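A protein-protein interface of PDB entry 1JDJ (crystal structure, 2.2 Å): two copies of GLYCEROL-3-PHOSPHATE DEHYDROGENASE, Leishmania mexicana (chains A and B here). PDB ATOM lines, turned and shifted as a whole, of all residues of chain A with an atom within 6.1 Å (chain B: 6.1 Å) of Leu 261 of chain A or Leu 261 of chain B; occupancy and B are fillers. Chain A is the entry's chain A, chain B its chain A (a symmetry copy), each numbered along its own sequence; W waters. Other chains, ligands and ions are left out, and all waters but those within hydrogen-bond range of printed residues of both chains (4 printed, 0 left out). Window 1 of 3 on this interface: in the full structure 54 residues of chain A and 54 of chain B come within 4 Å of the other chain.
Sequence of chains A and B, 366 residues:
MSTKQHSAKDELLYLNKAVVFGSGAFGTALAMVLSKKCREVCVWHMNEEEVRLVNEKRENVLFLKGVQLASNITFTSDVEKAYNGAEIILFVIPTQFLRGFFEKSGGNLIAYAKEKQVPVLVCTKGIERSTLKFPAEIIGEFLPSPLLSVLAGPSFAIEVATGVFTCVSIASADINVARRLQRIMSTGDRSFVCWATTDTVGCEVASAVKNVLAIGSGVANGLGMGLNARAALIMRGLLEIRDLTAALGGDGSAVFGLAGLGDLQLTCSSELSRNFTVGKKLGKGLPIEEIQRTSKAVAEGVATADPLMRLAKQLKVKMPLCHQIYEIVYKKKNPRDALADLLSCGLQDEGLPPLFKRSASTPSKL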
ATOM      1  N   PRO A 154      -3.892  12.024 -30.029  1.00  0.00           N
ATOM      2  CA  PRO A 154      -5.273  11.586 -29.786  1.00  0.00           C
ATOM      3  C   PRO A 154      -6.141  12.835 -29.852  1.00  0.00           C
ATOM      4  O   PRO A 154      -6.166  13.622 -28.902  1.00  0.00           O
ATOM      5  CB  PRO A 154      -5.226  11.020 -28.364  1.00  0.00           C
ATOM      6  CG  PRO A 154      -3.748  10.963 -28.001  1.00  0.00           C
ATOM      7  CD  PRO A 154      -3.140  12.089 -28.768  1.00  0.00           C
ATOM      8  N   ALA A 206       2.375   6.326 -37.867  1.00  0.00           N
ATOM      9  CA  ALA A 206       1.338   6.016 -36.887  1.00  0.00           C
ATOM     10  C   ALA A 206      -0.044   6.490 -37.349  1.00  0.00           C
ATOM     11  O   ALA A 206      -1.033   5.772 -37.202  1.00  0.00           O
ATOM     12  CB  ALA A 206       1.691   6.659 -35.531  1.00  0.00           C
ATOM     13  N   ALA A 231      -6.735  -4.574 -26.165  1.00  0.00           N
ATOM     14  CA  ALA A 231      -5.512  -4.064 -25.548  1.00  0.00           C
ATOM     15  C   ALA A 231      -4.282  -4.747 -26.154  1.00  0.00           C
ATOM     16  O   ALA A 231      -3.258  -4.105 -26.386  1.00  0.00           O
ATOM     17  CB  ALA A 231      -5.554  -4.294 -24.045  1.00  0.00           C
ATOM     18  N   ILE A 234      -3.582  -3.438 -29.726  1.00  0.00           N
ATOM     19  CA  ILE A 234      -2.969  -2.117 -29.665  1.00  0.00           C
ATOM     20  C   ILE A 234      -1.477  -2.216 -29.354  1.00  0.00           C
ATOM     21  O   ILE A 234      -0.652  -1.574 -30.012  1.00  0.00           O
ATOM     22  CB  ILE A 234      -3.634  -1.238 -28.574  1.00  0.00           C
ATOM     23  CG1 ILE A 234      -5.066  -0.888 -28.983  1.00  0.00           C
ATOM     24  CG2 ILE A 234      -2.833   0.027 -28.359  1.00  0.00           C
ATOM     25  CD1 ILE A 234      -5.844  -0.153 -27.901  1.00  0.00           C
ATOM     26  N   MET A 235      -1.144  -3.027 -28.352  1.00  0.00           N
ATOM     27  CA  MET A 235       0.236  -3.209 -27.918  1.00  0.00           C
ATOM     28  C   MET A 235       1.089  -3.888 -28.979  1.00  0.00           C
ATOM     29  O   MET A 235       2.199  -3.437 -29.258  1.00  0.00           O
ATOM     30  CB  MET A 235       0.264  -4.006 -26.603  1.00  0.00           C
ATOM     31  CG  MET A 235       1.634  -4.133 -25.912  1.00  0.00           C
ATOM     32  SD  MET A 235       2.675  -5.536 -26.456  1.00  0.00           S
ATOM     33  CE  MET A 235       4.068  -4.636 -27.207  1.00  0.00           C
ATOM     34  N   LEU A 238       1.350  -1.580 -32.193  1.00  0.00           N
ATOM     35  CA  LEU A 238       2.283  -0.469 -32.058  1.00  0.00           C
ATOM     36  C   LEU A 238       3.683  -0.869 -32.528  1.00  0.00           C
ATOM     37  O   LEU A 238       4.435  -0.036 -33.037  1.00  0.00           O
ATOM     38  CB  LEU A 238       2.338  -0.003 -30.597  1.00  0.00           C
ATOM     39  CG  LEU A 238       3.137   1.262 -30.285  1.00  0.00           C
ATOM     40  CD1 LEU A 238       2.604   2.432 -31.105  1.00  0.00           C
ATOM     41  CD2 LEU A 238       3.033   1.568 -28.800  1.00  0.00           C
ATOM     42  N   ALA A 254       8.478   9.291 -31.590  1.00  0.00           N
ATOM     43  CA  ALA A 254       7.038   9.556 -31.514  1.00  0.00           C
ATOM     44  C   ALA A 254       6.213   8.286 -31.313  1.00  0.00           C
ATOM     45  O   ALA A 254       5.058   8.348 -30.887  1.00  0.00           O
ATOM     46  CB  ALA A 254       6.562  10.267 -32.781  1.00  0.00           C
ATOM     47  N   VAL A 255       6.805   7.138 -31.615  1.00  0.00           N
ATOM     48  CA  VAL A 255       6.106   5.860 -31.498  1.00  0.00           C
ATOM     49  C   VAL A 255       5.382   5.625 -30.174  1.00  0.00           C
ATOM     50  O   VAL A 255       4.213   5.242 -30.159  1.00  0.00           O
ATOM     51  CB  VAL A 255       7.070   4.685 -31.744  1.00  0.00           C
ATOM     52  CG1 VAL A 255       6.376   3.365 -31.437  1.00  0.00           C
ATOM     53  CG2 VAL A 255       7.547   4.710 -33.182  1.00  0.00           C
ATOM     54  N   PHE A 256       6.071   5.842 -29.063  1.00  0.00           N
ATOM     55  CA  PHE A 256       5.449   5.621 -27.771  1.00  0.00           C
ATOM     56  C   PHE A 256       4.909   6.906 -27.155  1.00  0.00           C
ATOM     57  O   PHE A 256       4.708   6.990 -25.951  1.00  0.00           O
ATOM     58  CB  PHE A 256       6.447   4.935 -26.835  1.00  0.00           C
ATOM     59  CG  PHE A 256       6.882   3.581 -27.321  1.00  0.00           C
ATOM     60  CD1 PHE A 256       8.181   3.368 -27.770  1.00  0.00           C
ATOM     61  CD2 PHE A 256       5.979   2.527 -27.365  1.00  0.00           C
ATOM     62  CE1 PHE A 256       8.572   2.122 -28.255  1.00  0.00           C
ATOM     63  CE2 PHE A 256       6.362   1.276 -27.851  1.00  0.00           C
ATOM     64  CZ  PHE A 256       7.660   1.075 -28.296  1.00  0.00           C
ATOM     65  N   GLY A 257       4.679   7.905 -27.999  1.00  0.00           N
ATOM     66  CA  GLY A 257       4.151   9.169 -27.521  1.00  0.00           C
ATOM     67  C   GLY A 257       2.724   9.397 -27.987  1.00  0.00           C
ATOM     68  O   GLY A 257       2.040   8.460 -28.406  1.00  0.00           O
ATOM     69  N   LEU A 258       2.284  10.651 -27.930  1.00  0.00           N
ATOM     70  CA  LEU A 258       0.931  11.025 -28.319  1.00  0.00           C
ATOM     71  C   LEU A 258       0.518  10.613 -29.728  1.00  0.00           C
ATOM     72  O   LEU A 258      -0.568  10.075 -29.916  1.00  0.00           O
ATOM     73  CB  LEU A 258       0.747  12.536 -28.155  1.00  0.00           C
ATOM     74  CG  LEU A 258       0.763  13.044 -26.711  1.00  0.00           C
ATOM     75  CD1 LEU A 258       0.847  14.568 -26.693  1.00  0.00           C
ATOM     76  CD2 LEU A 258      -0.485  12.544 -25.990  1.00  0.00           C
ATOM     77  N   ALA A 259       1.373  10.866 -30.713  1.00  0.00           N
ATOM     78  CA  ALA A 259       1.067  10.516 -32.098  1.00  0.00           C
ATOM     79  C   ALA A 259       1.068   9.009 -32.322  1.00  0.00           C
ATOM     80  O   ALA A 259       0.375   8.501 -33.210  1.00  0.00           O
ATOM     81  CB  ALA A 259       2.068  11.181 -33.034  1.00  0.00           C
ATOM     82  N   GLY A 260       1.847   8.296 -31.516  1.00  0.00           N
ATOM     83  CA  GLY A 260       1.923   6.854 -31.648  1.00  0.00           C
ATOM     84  C   GLY A 260       0.869   6.115 -30.843  1.00  0.00           C
ATOM     85  O   GLY A 260      -0.289   6.030 -31.260  1.00  0.00           O
ATOM     86  N   LEU A 261       1.257   5.587 -29.683  1.00  0.00           N
ATOM     87  CA  LEU A 261       0.315   4.844 -28.854  1.00  0.00           C
ATOM     88  C   LEU A 261      -0.891   5.672 -28.405  1.00  0.00           C
ATOM     89  O   LEU A 261      -1.998   5.145 -28.287  1.00  0.00           O
ATOM     90  CB  LEU A 261       1.027   4.243 -27.629  1.00  0.00           C
ATOM     91  CG  LEU A 261       1.556   5.081 -26.461  1.00  0.00           C
ATOM     92  CD1 LEU A 261       0.415   5.669 -25.635  1.00  0.00           C
ATOM     93  CD2 LEU A 261       2.404   4.176 -25.578  1.00  0.00           C
ATOM     94  N   GLY A 262      -0.678   6.961 -28.164  1.00  0.00           N
ATOM     95  CA  GLY A 262      -1.773   7.817 -27.741  1.00  0.00           C
ATOM     96  C   GLY A 262      -2.923   7.810 -28.735  1.00  0.00           C
ATOM     97  O   GLY A 262      -4.051   7.454 -28.401  1.00  0.00           O
ATOM     98  N   ASP A 263      -2.628   8.198 -29.969  1.00  0.00           N
ATOM     99  CA  ASP A 263      -3.635   8.254 -31.016  1.00  0.00           C
ATOM    100  C   ASP A 263      -4.122   6.854 -31.395  1.00  0.00           C
ATOM    101  O   ASP A 263      -5.290   6.663 -31.719  1.00  0.00           O
ATOM    102  CB  ASP A 263      -3.050   8.963 -32.244  1.00  0.00           C
ATOM    103  CG  ASP A 263      -4.117   9.459 -33.210  1.00  0.00           C
ATOM    104  OD1 ASP A 263      -3.744   9.959 -34.288  1.00  0.00           O
ATOM    105  OD2 ASP A 263      -5.320   9.361 -32.898  1.00  0.00           O
ATOM    106  N   LEU A 264      -3.226   5.873 -31.345  1.00  0.00           N
ATOM    107  CA  LEU A 264      -3.585   4.503 -31.701  1.00  0.00           C
ATOM    108  C   LEU A 264      -4.632   3.898 -30.769  1.00  0.00           C
ATOM    109  O   LEU A 264      -5.626   3.341 -31.229  1.00  0.00           O
ATOM    110  CB  LEU A 264      -2.340   3.601 -31.711  1.00  0.00           C
ATOM    111  CG  LEU A 264      -2.617   2.118 -31.995  1.00  0.00           C
ATOM    112  CD1 LEU A 264      -3.172   1.958 -33.407  1.00  0.00           C
ATOM    113  CD2 LEU A 264      -1.332   1.300 -31.827  1.00  0.00           C
ATOM    114  N   GLN A 265      -4.414   4.008 -29.462  1.00  0.00           N
ATOM    115  CA  GLN A 265      -5.359   3.439 -28.509  1.00  0.00           C
ATOM    116  C   GLN A 265      -6.709   4.153 -28.607  1.00  0.00           C
ATOM    117  O   GLN A 265      -7.760   3.530 -28.480  1.00  0.00           O
ATOM    118  CB  GLN A 265      -4.785   3.494 -27.082  1.00  0.00           C
ATOM    119  CG  GLN A 265      -4.936   4.802 -26.341  1.00  0.00           C
ATOM    120  CD  GLN A 265      -6.326   4.983 -25.756  1.00  0.00           C
ATOM    121  OE1 GLN A 265      -6.912   4.050 -25.206  1.00  0.00           O
ATOM    122  NE2 GLN A 265      -6.853   6.194 -25.860  1.00  0.00           N
ATOM    123  N   LEU A 266      -6.682   5.454 -28.867  1.00  0.00           N
ATOM    124  CA  LEU A 266      -7.916   6.212 -29.007  1.00  0.00           C
ATOM    125  C   LEU A 266      -8.668   5.739 -30.250  1.00  0.00           C
ATOM    126  O   LEU A 266      -9.857   5.427 -30.195  1.00  0.00           O
ATOM    127  CB  LEU A 266      -7.611   7.706 -29.157  1.00  0.00           C
ATOM    128  CG  LEU A 266      -8.811   8.620 -29.433  1.00  0.00           C
ATOM    129  CD1 LEU A 266      -9.527   8.920 -28.133  1.00  0.00           C
ATOM    130  CD2 LEU A 266      -8.348   9.921 -30.073  1.00  0.00           C
ATOM    131  N   PRO B 154      -3.013  -7.002 -19.886  1.00  0.00           N
ATOM    132  CA  PRO B 154      -4.421  -6.589 -19.934  1.00  0.00           C
ATOM    133  C   PRO B 154      -5.249  -7.853 -19.750  1.00  0.00           C
ATOM    134  O   PRO B 154      -5.393  -8.642 -20.688  1.00  0.00           O
ATOM    135  CB  PRO B 154      -4.583  -6.024 -21.348  1.00  0.00           C
ATOM    136  CG  PRO B 154      -3.171  -5.941 -21.913  1.00  0.00           C
ATOM    137  CD  PRO B 154      -2.442  -7.055 -21.240  1.00  0.00           C
ATOM    138  N   ALA B 206       4.179  -1.182 -12.987  1.00  0.00           N
ATOM    139  CA  ALA B 206       3.010  -0.893 -13.814  1.00  0.00           C
ATOM    140  C   ALA B 206       1.715  -1.390 -13.165  1.00  0.00           C
ATOM    141  O   ALA B 206       0.702  -0.690 -13.172  1.00  0.00           O
ATOM    142  CB  ALA B 206       3.183  -1.530 -15.206  1.00  0.00           C
ATOM    143  N   ALA B 231      -6.661   9.538 -23.296  1.00  0.00           N
ATOM    144  CA  ALA B 231      -5.528   9.049 -24.078  1.00  0.00           C
ATOM    145  C   ALA B 231      -4.238   9.755 -23.648  1.00  0.00           C
ATOM    146  O   ALA B 231      -3.180   9.132 -23.561  1.00  0.00           O
ATOM    147  CB  ALA B 231      -5.782   9.276 -25.561  1.00  0.00           C
ATOM    148  N   ILE B 234      -3.024   8.463 -20.210  1.00  0.00           N
ATOM    149  CA  ILE B 234      -2.403   7.153 -20.357  1.00  0.00           C
ATOM    150  C   ILE B 234      -0.970   7.279 -20.872  1.00  0.00           C
ATOM    151  O   ILE B 234      -0.050   6.652 -20.336  1.00  0.00           O
ATOM    152  CB  ILE B 234      -3.197   6.261 -21.346  1.00  0.00           C
ATOM    153  CG1 ILE B 234      -4.552   5.885 -20.743  1.00  0.00           C
ATOM    154  CG2 ILE B 234      -2.411   5.010 -21.672  1.00  0.00           C
ATOM    155  CD1 ILE B 234      -5.459   5.136 -21.707  1.00  0.00           C
ATOM    156  N   MET B 235      -0.794   8.094 -21.909  1.00  0.00           N
ATOM    157  CA  MET B 235       0.509   8.300 -22.531  1.00  0.00           C
ATOM    158  C   MET B 235       1.488   8.995 -21.598  1.00  0.00           C
ATOM    159  O   MET B 235       2.634   8.565 -21.477  1.00  0.00           O
ATOM    160  CB  MET B 235       0.340   9.096 -23.837  1.00  0.00           C
ATOM    161  CG  MET B 235       1.597   9.246 -24.711  1.00  0.00           C
ATOM    162  SD  MET B 235       2.679  10.668 -24.315  1.00  0.00           S
ATOM    163  CE  MET B 235       4.178   9.795 -23.766  1.00  0.00           C
ATOM    164  N   LEU B 238       2.235   6.697 -18.454  1.00  0.00           N
ATOM    165  CA  LEU B 238       3.160   5.602 -18.719  1.00  0.00           C
ATOM    166  C   LEU B 238       4.604   6.027 -18.448  1.00  0.00           C
ATOM    167  O   LEU B 238       5.434   5.209 -18.049  1.00  0.00           O
ATOM    168  CB  LEU B 238       3.019   5.135 -20.174  1.00  0.00           C
ATOM    169  CG  LEU B 238       3.790   3.884 -20.596  1.00  0.00           C
ATOM    170  CD1 LEU B 238       3.397   2.707 -19.711  1.00  0.00           C
ATOM    171  CD2 LEU B 238       3.486   3.575 -22.052  1.00  0.00           C
ATOM    172  N   ALA B 254       9.403  -4.046 -20.055  1.00  0.00           N
ATOM    173  CA  ALA B 254       7.971  -4.336 -19.931  1.00  0.00           C
ATOM    174  C   ALA B 254       7.104  -3.082 -20.014  1.00  0.00           C
ATOM    175  O   ALA B 254       5.902  -3.165 -20.275  1.00  0.00           O
ATOM    176  CB  ALA B 254       7.689  -5.054 -18.611  1.00  0.00           C
ATOM    177  N   VAL B 255       7.712  -1.923 -19.795  1.00  0.00           N
ATOM    178  CA  VAL B 255       6.980  -0.658 -19.813  1.00  0.00           C
ATOM    179  C   VAL B 255       6.075  -0.437 -21.023  1.00  0.00           C
ATOM    180  O   VAL B 255       4.909  -0.075 -20.875  1.00  0.00           O
ATOM    181  CB  VAL B 255       7.948   0.534 -19.701  1.00  0.00           C
ATOM    182  CG1 VAL B 255       7.194   1.841 -19.908  1.00  0.00           C
ATOM    183  CG2 VAL B 255       8.620   0.520 -18.343  1.00  0.00           C
ATOM    184  N   PHE B 256       6.607  -0.643 -22.219  1.00  0.00           N
ATOM    185  CA  PHE B 256       5.808  -0.435 -23.412  1.00  0.00           C
ATOM    186  C   PHE B 256       5.211  -1.731 -23.948  1.00  0.00           C
ATOM    187  O   PHE B 256       4.846  -1.820 -25.113  1.00  0.00           O
ATOM    188  CB  PHE B 256       6.653   0.267 -24.477  1.00  0.00           C
ATOM    189  CG  PHE B 256       7.127   1.629 -24.054  1.00  0.00           C
ATOM    190  CD1 PHE B 256       8.473   1.866 -23.790  1.00  0.00           C
ATOM    191  CD2 PHE B 256       6.221   2.668 -23.884  1.00  0.00           C
ATOM    192  CE1 PHE B 256       8.904   3.119 -23.362  1.00  0.00           C
ATOM    193  CE2 PHE B 256       6.645   3.926 -23.454  1.00  0.00           C
ATOM    194  CZ  PHE B 256       7.989   4.150 -23.194  1.00  0.00           C
ATOM    195  N   GLY B 257       5.118  -2.733 -23.082  1.00  0.00           N
ATOM    196  CA  GLY B 257       4.551  -4.006 -23.483  1.00  0.00           C
ATOM    197  C   GLY B 257       3.207  -4.259 -22.824  1.00  0.00           C
ATOM    198  O   GLY B 257       2.572  -3.335 -22.313  1.00  0.00           O
ATOM    199  N   LEU B 258       2.786  -5.521 -22.821  1.00  0.00           N
ATOM    200  CA  LEU B 258       1.507  -5.919 -22.248  1.00  0.00           C
ATOM    201  C   LEU B 258       1.287  -5.512 -20.795  1.00  0.00           C
ATOM    202  O   LEU B 258       0.228  -4.994 -20.458  1.00  0.00           O
ATOM    203  CB  LEU B 258       1.330  -7.433 -22.387  1.00  0.00           C
ATOM    204  CG  LEU B 258       1.154  -7.942 -23.820  1.00  0.00           C
ATOM    205  CD1 LEU B 258       1.262  -9.464 -23.851  1.00  0.00           C
ATOM    206  CD2 LEU B 258      -0.192  -7.465 -24.360  1.00  0.00           C
ATOM    207  N   ALA B 259       2.275  -5.749 -19.939  1.00  0.00           N
ATOM    208  CA  ALA B 259       2.158  -5.403 -18.525  1.00  0.00           C
ATOM    209  C   ALA B 259       2.163  -3.895 -18.301  1.00  0.00           C
ATOM    210  O   ALA B 259       1.591  -3.399 -17.325  1.00  0.00           O
ATOM    211  CB  ALA B 259       3.291  -6.049 -17.737  1.00  0.00           C
ATOM    212  N   GLY B 260       2.810  -3.170 -19.206  1.00  0.00           N
ATOM    213  CA  GLY B 260       2.877  -1.726 -19.084  1.00  0.00           C
ATOM    214  C   GLY B 260       1.709  -1.007 -19.734  1.00  0.00           C
ATOM    215  O   GLY B 260       0.618  -0.942 -19.160  1.00  0.00           O
ATOM    216  N   LEU B 261       1.922  -0.475 -20.936  1.00  0.00           N
ATOM    217  CA  LEU B 261       0.861   0.251 -21.625  1.00  0.00           C
ATOM    218  C   LEU B 261      -0.381  -0.599 -21.903  1.00  0.00           C
ATOM    219  O   LEU B 261      -1.503  -0.093 -21.866  1.00  0.00           O
ATOM    220  CB  LEU B 261       1.385   0.863 -22.936  1.00  0.00           C
ATOM    221  CG  LEU B 261       1.761   0.033 -24.167  1.00  0.00           C
ATOM    222  CD1 LEU B 261       0.528  -0.576 -24.828  1.00  0.00           C
ATOM    223  CD2 LEU B 261       2.462   0.952 -25.158  1.00  0.00           C
ATOM    224  N   GLY B 262      -0.181  -1.884 -22.173  1.00  0.00           N
ATOM    225  CA  GLY B 262      -1.308  -2.760 -22.441  1.00  0.00           C
ATOM    226  C   GLY B 262      -2.308  -2.773 -21.297  1.00  0.00           C
ATOM    227  O   GLY B 262      -3.479  -2.437 -21.470  1.00  0.00           O
ATOM    228  N   ASP B 263      -1.838  -3.154 -20.116  1.00  0.00           N
ATOM    229  CA  ASP B 263      -2.689  -3.227 -18.939  1.00  0.00           C
ATOM    230  C   ASP B 263      -3.143  -1.835 -18.495  1.00  0.00           C
ATOM    231  O   ASP B 263      -4.259  -1.664 -18.012  1.00  0.00           O
ATOM    232  CB  ASP B 263      -1.926  -3.924 -17.805  1.00  0.00           C
ATOM    233  CG  ASP B 263      -2.839  -4.437 -16.701  1.00  0.00           C
ATOM    234  OD1 ASP B 263      -2.311  -4.929 -15.686  1.00  0.00           O
ATOM    235  OD2 ASP B 263      -4.076  -4.361 -16.844  1.00  0.00           O
ATOM    236  N   LEU B 264      -2.280  -0.838 -18.668  1.00  0.00           N
ATOM    237  CA  LEU B 264      -2.611   0.525 -18.264  1.00  0.00           C
ATOM    238  C   LEU B 264      -3.788   1.110 -19.040  1.00  0.00           C
ATOM    239  O   LEU B 264      -4.718   1.650 -18.446  1.00  0.00           O
ATOM    240  CB  LEU B 264      -1.394   1.450 -18.425  1.00  0.00           C
ATOM    241  CG  LEU B 264      -1.654   2.928 -18.104  1.00  0.00           C
ATOM    242  CD1 LEU B 264      -2.011   3.080 -16.628  1.00  0.00           C
ATOM    243  CD2 LEU B 264      -0.420   3.769 -18.448  1.00  0.00           C
ATOM    244  N   GLN B 265      -3.751   1.003 -20.365  1.00  0.00           N
ATOM    245  CA  GLN B 265      -4.830   1.553 -21.177  1.00  0.00           C
ATOM    246  C   GLN B 265      -6.141   0.816 -20.893  1.00  0.00           C
ATOM    247  O   GLN B 265      -7.210   1.419 -20.872  1.00  0.00           O
ATOM    248  CB  GLN B 265      -4.459   1.507 -22.670  1.00  0.00           C
ATOM    249  CG  GLN B 265      -4.689   0.195 -23.384  1.00  0.00           C
ATOM    250  CD  GLN B 265      -6.142  -0.011 -23.771  1.00  0.00           C
ATOM    251  OE1 GLN B 265      -6.816   0.911 -24.233  1.00  0.00           O
ATOM    252  NE2 GLN B 265      -6.628  -1.231 -23.596  1.00  0.00           N
ATOM    253  N   LEU B 266      -6.054  -0.484 -20.641  1.00  0.00           N
ATOM    254  CA  LEU B 266      -7.243  -1.264 -20.332  1.00  0.00           C
ATOM    255  C   LEU B 266      -7.824  -0.803 -18.996  1.00  0.00           C
ATOM    256  O   LEU B 266      -9.014  -0.512 -18.885  1.00  0.00           O
ATOM    257  CB  LEU B 266      -6.894  -2.752 -20.227  1.00  0.00           C
ATOM    258  CG  LEU B 266      -8.027  -3.688 -19.789  1.00  0.00           C
ATOM    259  CD1 LEU B 266      -8.911  -4.002 -20.977  1.00  0.00           C
ATOM    260  CD2 LEU B 266      -7.456  -4.978 -19.221  1.00  0.00           C
HETATM  261  O   HOH W   1       3.981  -1.266 -27.759  1.00  0.00           O
HETATM  262  O   HOH W   2      -8.983   7.481 -24.614  1.00  0.00           O
HETATM  263  O   HOH W   3       4.229   6.424 -23.211  1.00  0.00           O
HETATM  264  O   HOH W   4      -8.887  -2.558 -24.535  1.00  0.00           O
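Of the printed residues of chain B, Phe 256 of chain A touches Met 235 and Phe 256. Leu 266 of chain A touches none of the printed residues of chain B. Printed residues of chain A within 4 Å of Leu 238 of chain B: Leu 261 (3.7 Å). Of the printed residues of chain A, Leu 258 of chain B touches Met 235. Of chain A, only Met 235, Leu 238 and Leu 261 come within 4 Å of Leu 261 of chain B. Of the printed residues of chain A, Gly 262 of chain B touches Ala 231. Asp 263 of chain B touches none of the printed residues of chain A. The nearest printed residue of chain B that does not touch Ile 234 of chain A is Leu 261 of chain B (4.9 Å).
Water W2 bridges NE2 of Gln 265 of chain A (2.8 Å) and N of Ala 231 of chain B (3.4 Å). Water W4 lies within hydrogen-bond range of the side-chain amide nitrogen of Gln 265 of chain B (2.8 Å) and the backbone NH of Ala 231 of chain A (3.4 Å). Water W1 bridges O of Phe 256 of chain B (2.8 Å) and O of Met 235 of chain A (3.2 Å). Water W3 lies within hydrogen-bond range of O of Phe 256 of chain A (2.8 Å) and O of Met 235 of chain B (3.2 Å).
The side-chain sulfur of Met 235 of chain A lies close to the backbone NH of Leu 258 of chain B (3.6 Å). N of Leu 258 of chain A lies close to SD of Met 235 of chain B. The side-chain amide oxygen (OE1) of Gln 265 of chain A lies close to the side-chain amide oxygen (OE1) of Gln 265 of chain B, 3.3 Å away.
Among the printed residues, pairs that only touch across the chains: Pro 154 of chain A with Ala 231 of chain B (3.3 Å), Ala 231 of chain A with Pro 154 of chain B (3.3 Å), Ala 231 of chain A with Gly 262 of chain B (3.8 Å), Ala 231 of chain A with Gln 265 of chain B (3.3 Å), Ile 234 of chain A with Gln 265 of chain B (3.9 Å), Met 235 of chain A with Phe 256 of chain B (3.6 Å), Met 235 of chain A with Gly 257 of chain B (3.5 Å), Met 235 of chain A with Leu 261 of chain B (3.9 Å), Leu 238 of chain A with Leu 261 of chain B (3.7 Å), Phe 256 of chain A with Met 235 of chain B (3.6 Å), Phe 256 of chain A with Phe 256 of chain B (3.5 Å), Gly 257 of chain A with Met 235 of chain B (3.5 Å), Leu 261 of chain A with Met 235 of chain B (3.9 Å), Leu 261 of chain A with Leu 238 of chain B (3.7 Å), Leu 261 of chain A with Leu 261 of chain B (3.3 Å), Gly 262 of chain A with Ala 231 of chain B (3.8 Å), Gln 265 of chain A with Ala 231 of chain B (3.3 Å) and Gln 265 of chain A with Ile 234 of chain B (3.9 Å).
Along chain A the printed residues that touch a printed residue of chain B span positions 154 to 265. Hydrophobic or aromatic side chains of chain B within 4 Å of the printed part of chain A: Pro 154, Ala 231, Ile 234, Met 235, Leu 238, Phe 256, Leu 258 and Leu 261.
The backbone NH (N) of Leu 261 of chain A lies within hydrogen-bond range of the backbone carbonyl oxygen (O) of Val 255 of chain A (3.0 Å). O of Gly 257 of chain A lies within hydrogen-bond range of N of Gly 262 of chain A (3.1 Å). The backbone NH of Asp 263 of chain A lies within hydrogen-bond range of the backbone carbonyl oxygen of Leu 258 of chain A. The backbone carbonyl oxygen (O) of Val 255 of chain B is in hydrogen-bond range of the backbone NH (N) of Leu 261 of chain B (3.0 Å). The backbone carbonyl oxygen (O) of Gly 257 of chain B is in hydrogen-bond range of the backbone NH (N) of Gly 262 of chain B (3.1 Å). The backbone carbonyl oxygen (O) of Leu 258 of chain B lies within hydrogen-bond range of the backbone NH (N) of Asp 263 of chain B, at 2.8 Å.
Pro 154 of chain A touches Ala 231 of chain B, and with the chains exchanged Ala 231 of chain A touches Pro 154 of chain B. Ala 231 of chain A touches Gly 262 of chain B, and with the chains exchanged Gly 262 of chain A touches Ala 231 of chain B. Met 235 of chain A touches Gly 257 of chain B, and with the chains exchanged Gly 257 of chain A touches Met 235 of chain B. Gln 265 of chain B touches its own counterpart, Gln 265 of chain A. Of the 21 pairs that touch across the chains among the printed residues, 21 have their exchanged pair printed and touching as well.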
